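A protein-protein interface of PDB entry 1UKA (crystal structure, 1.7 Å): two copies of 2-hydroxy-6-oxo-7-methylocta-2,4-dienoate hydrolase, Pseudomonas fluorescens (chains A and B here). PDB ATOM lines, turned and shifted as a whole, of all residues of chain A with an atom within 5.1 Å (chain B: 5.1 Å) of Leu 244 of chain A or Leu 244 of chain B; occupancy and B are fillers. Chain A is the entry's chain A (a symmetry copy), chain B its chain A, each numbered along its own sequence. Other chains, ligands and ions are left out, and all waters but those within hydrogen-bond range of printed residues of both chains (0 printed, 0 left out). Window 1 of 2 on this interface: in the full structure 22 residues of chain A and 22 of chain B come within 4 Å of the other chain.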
ATOM      1  N   LEU A 217     -30.100 -21.076   3.128  1.00  0.00           N
ATOM      2  CA  LEU A 217     -30.227 -19.642   2.909  1.00  0.00           C
ATOM      3  C   LEU A 217     -30.209 -19.000   4.292  1.00  0.00           C
ATOM      4  O   LEU A 217     -31.085 -19.254   5.114  1.00  0.00           O
ATOM      5  CB  LEU A 217     -31.542 -19.316   2.189  1.00  0.00           C
ATOM      6  CG  LEU A 217     -31.910 -17.830   2.075  1.00  0.00           C
ATOM      7  CD1 LEU A 217     -30.832 -17.065   1.321  1.00  0.00           C
ATOM      8  CD2 LEU A 217     -33.255 -17.705   1.367  1.00  0.00           C
ATOM      9  N   ILE A 218     -29.190 -18.187   4.547  1.00  0.00           N
ATOM     10  CA  ILE A 218     -29.037 -17.514   5.832  1.00  0.00           C
ATOM     11  C   ILE A 218     -29.484 -16.068   5.663  1.00  0.00           C
ATOM     12  O   ILE A 218     -28.973 -15.356   4.804  1.00  0.00           O
ATOM     13  CB  ILE A 218     -27.565 -17.554   6.283  1.00  0.00           C
ATOM     14  CG1 ILE A 218     -27.066 -19.003   6.280  1.00  0.00           C
ATOM     15  CG2 ILE A 218     -27.428 -16.956   7.677  1.00  0.00           C
ATOM     16  CD1 ILE A 218     -25.555 -19.125   6.367  1.00  0.00           C
ATOM     17  N   ILE A 219     -30.446 -15.647   6.480  1.00  0.00           N
ATOM     18  CA  ILE A 219     -30.993 -14.295   6.421  1.00  0.00           C
ATOM     19  C   ILE A 219     -30.769 -13.565   7.743  1.00  0.00           C
ATOM     20  O   ILE A 219     -30.919 -14.150   8.816  1.00  0.00           O
ATOM     21  CB  ILE A 219     -32.505 -14.347   6.117  1.00  0.00           C
ATOM     22  CG1 ILE A 219     -32.728 -15.015   4.757  1.00  0.00           C
ATOM     23  CG2 ILE A 219     -33.101 -12.946   6.141  1.00  0.00           C
ATOM     24  CD1 ILE A 219     -34.193 -15.224   4.403  1.00  0.00           C
ATOM     25  N   HIS A 220     -30.417 -12.285   7.666  1.00  0.00           N
ATOM     26  CA  HIS A 220     -30.166 -11.504   8.873  1.00  0.00           C
ATOM     27  C   HIS A 220     -30.417 -10.020   8.625  1.00  0.00           C
ATOM     28  O   HIS A 220     -30.206  -9.523   7.520  1.00  0.00           O
ATOM     29  CB  HIS A 220     -28.711 -11.700   9.323  1.00  0.00           C
ATOM     30  CG  HIS A 220     -28.512 -11.625  10.807  1.00  0.00           C
ATOM     31  ND1 HIS A 220     -28.274 -12.740  11.579  1.00  0.00           N
ATOM     32  CD2 HIS A 220     -28.528 -10.573  11.660  1.00  0.00           C
ATOM     33  CE1 HIS A 220     -28.149 -12.379  12.845  1.00  0.00           C
ATOM     34  NE2 HIS A 220     -28.298 -11.069  12.920  1.00  0.00           N
ATOM     35  N   SER A 232     -24.405 -14.786  11.871  1.00  0.00           N
ATOM     36  CA  SER A 232     -24.819 -15.304  10.572  1.00  0.00           C
ATOM     37  C   SER A 232     -23.665 -15.291   9.582  1.00  0.00           C
ATOM     38  O   SER A 232     -23.614 -16.121   8.676  1.00  0.00           O
ATOM     39  CB  SER A 232     -25.999 -14.509  10.018  1.00  0.00           C
ATOM     40  OG  SER A 232     -27.198 -14.940  10.633  1.00  0.00           O
ATOM     41  N   LEU A 233     -22.741 -14.347   9.747  1.00  0.00           N
ATOM     42  CA  LEU A 233     -21.585 -14.298   8.864  1.00  0.00           C
ATOM     43  C   LEU A 233     -20.787 -15.571   9.121  1.00  0.00           C
ATOM     44  O   LEU A 233     -20.251 -16.184   8.196  1.00  0.00           O
ATOM     45  CB  LEU A 233     -20.720 -13.068   9.162  1.00  0.00           C
ATOM     46  CG  LEU A 233     -21.345 -11.699   8.883  1.00  0.00           C
ATOM     47  CD1 LEU A 233     -20.368 -10.599   9.267  1.00  0.00           C
ATOM     48  CD2 LEU A 233     -21.708 -11.595   7.412  1.00  0.00           C
ATOM     49  N   ALA A 242     -24.203 -22.581   1.167  1.00  0.00           N
ATOM     50  CA  ALA A 242     -24.953 -21.494   1.766  1.00  0.00           C
ATOM     51  C   ALA A 242     -24.934 -20.185   0.999  1.00  0.00           C
ATOM     52  O   ALA A 242     -23.995 -19.877   0.268  1.00  0.00           O
ATOM     53  CB  ALA A 242     -24.448 -21.247   3.181  1.00  0.00           C
ATOM     54  N   GLN A 243     -26.010 -19.431   1.176  1.00  0.00           N
ATOM     55  CA  GLN A 243     -26.145 -18.106   0.603  1.00  0.00           C
ATOM     56  C   GLN A 243     -26.485 -17.260   1.816  1.00  0.00           C
ATOM     57  O   GLN A 243     -27.216 -17.707   2.701  1.00  0.00           O
ATOM     58  CB  GLN A 243     -27.305 -18.023  -0.382  1.00  0.00           C
ATOM     59  CG  GLN A 243     -27.114 -18.783  -1.670  1.00  0.00           C
ATOM     60  CD  GLN A 243     -28.321 -18.645  -2.567  1.00  0.00           C
ATOM     61  OE1 GLN A 243     -28.540 -17.597  -3.181  1.00  0.00           O
ATOM     62  NE2 GLN A 243     -29.130 -19.695  -2.631  1.00  0.00           N
ATOM     63  N   LEU A 244     -25.946 -16.052   1.868  1.00  0.00           N
ATOM     64  CA  LEU A 244     -26.221 -15.147   2.970  1.00  0.00           C
ATOM     65  C   LEU A 244     -26.916 -13.917   2.409  1.00  0.00           C
ATOM     66  O   LEU A 244     -26.461 -13.338   1.424  1.00  0.00           O
ATOM     67  CB  LEU A 244     -24.918 -14.725   3.653  1.00  0.00           C
ATOM     68  CG  LEU A 244     -25.012 -13.613   4.707  1.00  0.00           C
ATOM     69  CD1 LEU A 244     -25.825 -14.090   5.906  1.00  0.00           C
ATOM     70  CD2 LEU A 244     -23.608 -13.218   5.146  1.00  0.00           C
ATOM     71  N   HIS A 245     -28.033 -13.530   3.013  1.00  0.00           N
ATOM     72  CA  HIS A 245     -28.721 -12.334   2.557  1.00  0.00           C
ATOM     73  C   HIS A 245     -28.949 -11.447   3.764  1.00  0.00           C
ATOM     74  O   HIS A 245     -29.667 -11.814   4.697  1.00  0.00           O
ATOM     75  CB  HIS A 245     -30.062 -12.656   1.901  1.00  0.00           C
ATOM     76  CG  HIS A 245     -30.625 -11.512   1.113  1.00  0.00           C
ATOM     77  ND1 HIS A 245     -30.379 -11.343  -0.233  1.00  0.00           N
ATOM     78  CD2 HIS A 245     -31.376 -10.452   1.493  1.00  0.00           C
ATOM     79  CE1 HIS A 245     -30.956 -10.230  -0.649  1.00  0.00           C
ATOM     80  NE2 HIS A 245     -31.568  -9.670   0.380  1.00  0.00           N
ATOM     81  N   VAL A 246     -28.312 -10.282   3.744  1.00  0.00           N
ATOM     82  CA  VAL A 246     -28.425  -9.326   4.832  1.00  0.00           C
ATOM     83  C   VAL A 246     -29.283  -8.152   4.388  1.00  0.00           C
ATOM     84  O   VAL A 246     -29.021  -7.535   3.356  1.00  0.00           O
ATOM     85  CB  VAL A 246     -27.034  -8.801   5.252  1.00  0.00           C
ATOM     86  CG1 VAL A 246     -27.174  -7.800   6.395  1.00  0.00           C
ATOM     87  CG2 VAL A 246     -26.149  -9.966   5.675  1.00  0.00           C
ATOM     88  N   LEU B 217     -28.031  -3.171  -4.087  1.00  0.00           N
ATOM     89  CA  LEU B 217     -27.914  -4.608  -3.878  1.00  0.00           C
ATOM     90  C   LEU B 217     -26.442  -4.946  -4.081  1.00  0.00           C
ATOM     91  O   LEU B 217     -25.899  -4.760  -5.167  1.00  0.00           O
ATOM     92  CB  LEU B 217     -28.781  -5.377  -4.882  1.00  0.00           C
ATOM     93  CG  LEU B 217     -28.601  -6.901  -4.917  1.00  0.00           C
ATOM     94  CD1 LEU B 217     -28.914  -7.510  -3.558  1.00  0.00           C
ATOM     95  CD2 LEU B 217     -29.512  -7.484  -5.993  1.00  0.00           C
ATOM     96  N   ILE B 218     -25.798  -5.421  -3.022  1.00  0.00           N
ATOM     97  CA  ILE B 218     -24.383  -5.776  -3.068  1.00  0.00           C
ATOM     98  C   ILE B 218     -24.281  -7.293  -3.170  1.00  0.00           C
ATOM     99  O   ILE B 218     -24.820  -8.010  -2.334  1.00  0.00           O
ATOM    100  CB  ILE B 218     -23.671  -5.293  -1.791  1.00  0.00           C
ATOM    101  CG1 ILE B 218     -23.927  -3.795  -1.596  1.00  0.00           C
ATOM    102  CG2 ILE B 218     -22.175  -5.559  -1.894  1.00  0.00           C
ATOM    103  CD1 ILE B 218     -23.572  -3.294  -0.207  1.00  0.00           C
ATOM    104  N   ILE B 219     -23.596  -7.769  -4.207  1.00  0.00           N
ATOM    105  CA  ILE B 219     -23.432  -9.199  -4.450  1.00  0.00           C
ATOM    106  C   ILE B 219     -21.954  -9.583  -4.427  1.00  0.00           C
ATOM    107  O   ILE B 219     -21.109  -8.857  -4.950  1.00  0.00           O
ATOM    108  CB  ILE B 219     -24.035  -9.577  -5.820  1.00  0.00           C
ATOM    109  CG1 ILE B 219     -25.534  -9.258  -5.821  1.00  0.00           C
ATOM    110  CG2 ILE B 219     -23.790 -11.050  -6.121  1.00  0.00           C
ATOM    111  CD1 ILE B 219     -26.213  -9.486  -7.163  1.00  0.00           C
ATOM    112  N   HIS B 220     -21.645 -10.729  -3.827  1.00  0.00           N
ATOM    113  CA  HIS B 220     -20.258 -11.178  -3.740  1.00  0.00           C
ATOM    114  C   HIS B 220     -20.182 -12.697  -3.630  1.00  0.00           C
ATOM    115  O   HIS B 220     -21.068 -13.331  -3.058  1.00  0.00           O
ATOM    116  CB  HIS B 220     -19.589 -10.551  -2.509  1.00  0.00           C
ATOM    117  CG  HIS B 220     -18.123 -10.287  -2.676  1.00  0.00           C
ATOM    118  ND1 HIS B 220     -17.613  -9.020  -2.858  1.00  0.00           N
ATOM    119  CD2 HIS B 220     -17.060 -11.127  -2.701  1.00  0.00           C
ATOM    120  CE1 HIS B 220     -16.299  -9.089  -2.986  1.00  0.00           C
ATOM    121  NE2 HIS B 220     -15.938 -10.356  -2.894  1.00  0.00           N
ATOM    122  N   SER B 232     -17.061  -6.076   0.347  1.00  0.00           N
ATOM    123  CA  SER B 232     -18.502  -5.936   0.178  1.00  0.00           C
ATOM    124  C   SER B 232     -19.208  -5.858   1.523  1.00  0.00           C
ATOM    125  O   SER B 232     -20.260  -5.231   1.638  1.00  0.00           O
ATOM    126  CB  SER B 232     -19.071  -7.085  -0.650  1.00  0.00           C
ATOM    127  OG  SER B 232     -18.832  -6.850  -2.025  1.00  0.00           O
ATOM    128  N   LEU B 233     -18.637  -6.498   2.540  1.00  0.00           N
ATOM    129  CA  LEU B 233     -19.231  -6.433   3.868  1.00  0.00           C
ATOM    130  C   LEU B 233     -19.138  -4.979   4.315  1.00  0.00           C
ATOM    131  O   LEU B 233     -20.058  -4.444   4.936  1.00  0.00           O
ATOM    132  CB  LEU B 233     -18.475  -7.333   4.851  1.00  0.00           C
ATOM    133  CG  LEU B 233     -18.531  -8.841   4.591  1.00  0.00           C
ATOM    134  CD1 LEU B 233     -17.704  -9.574   5.635  1.00  0.00           C
ATOM    135  CD2 LEU B 233     -19.975  -9.311   4.634  1.00  0.00           C
ATOM    136  N   ALA B 242     -29.078  -0.681   1.708  1.00  0.00           N
ATOM    137  CA  ALA B 242     -28.395  -1.782   1.056  1.00  0.00           C
ATOM    138  C   ALA B 242     -28.800  -3.169   1.518  1.00  0.00           C
ATOM    139  O   ALA B 242     -29.230  -3.374   2.651  1.00  0.00           O
ATOM    140  CB  ALA B 242     -26.891  -1.620   1.230  1.00  0.00           C
ATOM    141  N   GLN B 243     -28.664  -4.114   0.598  1.00  0.00           N
ATOM    142  CA  GLN B 243     -28.912  -5.517   0.868  1.00  0.00           C
ATOM    143  C   GLN B 243     -27.622  -6.170   0.406  1.00  0.00           C
ATOM    144  O   GLN B 243     -27.038  -5.753  -0.595  1.00  0.00           O
ATOM    145  CB  GLN B 243     -30.058  -6.068   0.029  1.00  0.00           C
ATOM    146  CG  GLN B 243     -31.427  -5.547   0.386  1.00  0.00           C
ATOM    147  CD  GLN B 243     -32.486  -6.146  -0.510  1.00  0.00           C
ATOM    148  OE1 GLN B 243     -32.858  -7.314  -0.362  1.00  0.00           O
ATOM    149  NE2 GLN B 243     -32.965  -5.357  -1.464  1.00  0.00           N
ATOM    150  N   LEU B 244     -27.171  -7.177   1.137  1.00  0.00           N
ATOM    151  CA  LEU B 244     -25.960  -7.892   0.775  1.00  0.00           C
ATOM    152  C   LEU B 244     -26.331  -9.338   0.493  1.00  0.00           C
ATOM    153  O   LEU B 244     -27.034  -9.967   1.282  1.00  0.00           O
ATOM    154  CB  LEU B 244     -24.947  -7.844   1.923  1.00  0.00           C
ATOM    155  CG  LEU B 244     -23.695  -8.720   1.785  1.00  0.00           C
ATOM    156  CD1 LEU B 244     -22.836  -8.233   0.622  1.00  0.00           C
ATOM    157  CD2 LEU B 244     -22.901  -8.669   3.084  1.00  0.00           C
ATOM    158  N   HIS B 245     -25.887  -9.862  -0.643  1.00  0.00           N
ATOM    159  CA  HIS B 245     -26.166 -11.254  -0.952  1.00  0.00           C
ATOM    160  C   HIS B 245     -24.850 -11.920  -1.298  1.00  0.00           C
ATOM    161  O   HIS B 245     -24.198 -11.567  -2.284  1.00  0.00           O
ATOM    162  CB  HIS B 245     -27.135 -11.402  -2.123  1.00  0.00           C
ATOM    163  CG  HIS B 245     -27.716 -12.778  -2.240  1.00  0.00           C
ATOM    164  ND1 HIS B 245     -28.904 -13.138  -1.638  1.00  0.00           N
ATOM    165  CD2 HIS B 245     -27.248 -13.895  -2.843  1.00  0.00           C
ATOM    166  CE1 HIS B 245     -29.142 -14.417  -1.867  1.00  0.00           C
ATOM    167  NE2 HIS B 245     -28.152 -14.900  -2.597  1.00  0.00           N
ATOM    168  N   VAL B 246     -24.458 -12.876  -0.465  1.00  0.00           N
ATOM    169  CA  VAL B 246     -23.214 -13.602  -0.659  1.00  0.00           C
ATOM    170  C   VAL B 246     -23.521 -15.013  -1.136  1.00  0.00           C
ATOM    171  O   VAL B 246     -24.297 -15.735  -0.511  1.00  0.00           O
ATOM    172  CB  VAL B 246     -22.410 -13.682   0.657  1.00  0.00           C
ATOM    173  CG1 VAL B 246     -21.109 -14.447   0.432  1.00  0.00           C
ATOM    174  CG2 VAL B 246     -22.115 -12.277   1.167  1.00  0.00           C
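N of Val 246 of chain A sits at hydrogen-bond distance from O of Leu 244 of chain B, at 2.8 Å.
N of Val 246 of chain B sits at hydrogen-bond distance from O of Leu 244 of chain A (2.8 Å).
A ring nitrogen (NE2) of His 245 of chain B lies within hydrogen-bond range of the side-chain amide oxygen (OE1) of Gln 243 of chain A (2.8 Å).
A ring nitrogen (ND1) of His 245 of chain A is in hydrogen-bond range of a ring nitrogen (ND1) of His 245 of chain B (2.7 Å).
The backbone carbonyl oxygen of Leu 244 of chain B sits close to the backbone carbonyl oxygen of Leu 244 of chain A, 3.4 Å away.
The side-chain amide oxygen (OE1) of Gln 243 of chain B sits at hydrogen-bond distance from a ring nitrogen (NE2) of His 245 of chain A, 2.8 Å away.
The backbone NH (N) of His 245 of chain A lies within hydrogen-bond range of the backbone carbonyl oxygen (O) of Ile 218 of chain A, 2.7 Å away.
The backbone carbonyl oxygen (O) of Gln 243 of chain A is in hydrogen-bond range of the backbone NH (N) of Ile 218 of chain A (2.7 Å).
The backbone carbonyl oxygen of His 245 of chain A sits at hydrogen-bond distance from the backbone NH of His 220 of chain A, 3.1 Å away.
The backbone NH (N) of Ile 218 of chain B is in hydrogen-bond range of the backbone carbonyl oxygen (O) of Gln 243 of chain B, at 2.7 Å.
The backbone carbonyl oxygen (O) of Ile 218 of chain B lies within hydrogen-bond range of the backbone NH (N) of His 245 of chain B, at 2.7 Å.
N of His 220 of chain B sits at hydrogen-bond distance from O of His 245 of chain B (3.1 Å).
Among the printed residues, merely in contact across the chains: His 245 of chain A with Leu 244 of chain B, Leu 244 of chain A with His 245 of chain B, Val 246 of chain A with Gln 243 of chain B, Gln 243 of chain A with Val 246 of chain B and Leu 233 of chain A with Leu 233 of chain B.
Of the printed residues of chain B, Leu 233 of chain A touches Leu 233.
Of the printed residues of chain B, Gln 243 of chain A touches His 245 (2.8 Å) and Val 246 (3.2 Å).
Leu 244 of chain A touches three residues of chain B.
Printed residues of chain B within 4 Å of Val 246 of chain A: Gln 243 (3.2 Å) and Leu 244 (2.8 Å).
Of the printed residues of chain A, Gln 243 of chain B touches His 245 and Val 246.
Of chain A, only Leu 244 (3.4 Å), His 245 (3.2 Å) and Val 246 (2.8 Å) come within 4 Å of Leu 244 of chain B.
Of the printed residues of chain A, His 245 of chain B touches Gln 243, Leu 244 and His 245.
The nearest printed residue of chain B that does not touch Leu 244 of chain A is Leu 233 of chain B (5.4 Å).
Hydrophobic or aromatic side chains of chain A that line the printed part of chain B: Leu 233 and His 245.
Of the 11 printed residues of chain B, 5 touch a printed residue of chain A.
Hydrophobic or aromatic side chains of chain B that line the printed part of chain A: Leu 233 and His 245.
Among the printed residues, 11 pairs touch across the chains.
Leu 233 of chain B touches its own counterpart, Leu 233 of chain A.
Leu 244 of chain B touches its own counterpart, Leu 244 of chain A.
Leu 244 of chain A touches His 245 of chain B, and with the chains exchanged His 245 of chain A touches Leu 244 of chain B.
Leu 244 of chain A touches Val 246 of chain B, and with the chains exchanged Val 246 of chain A touches Leu 244 of chain B.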
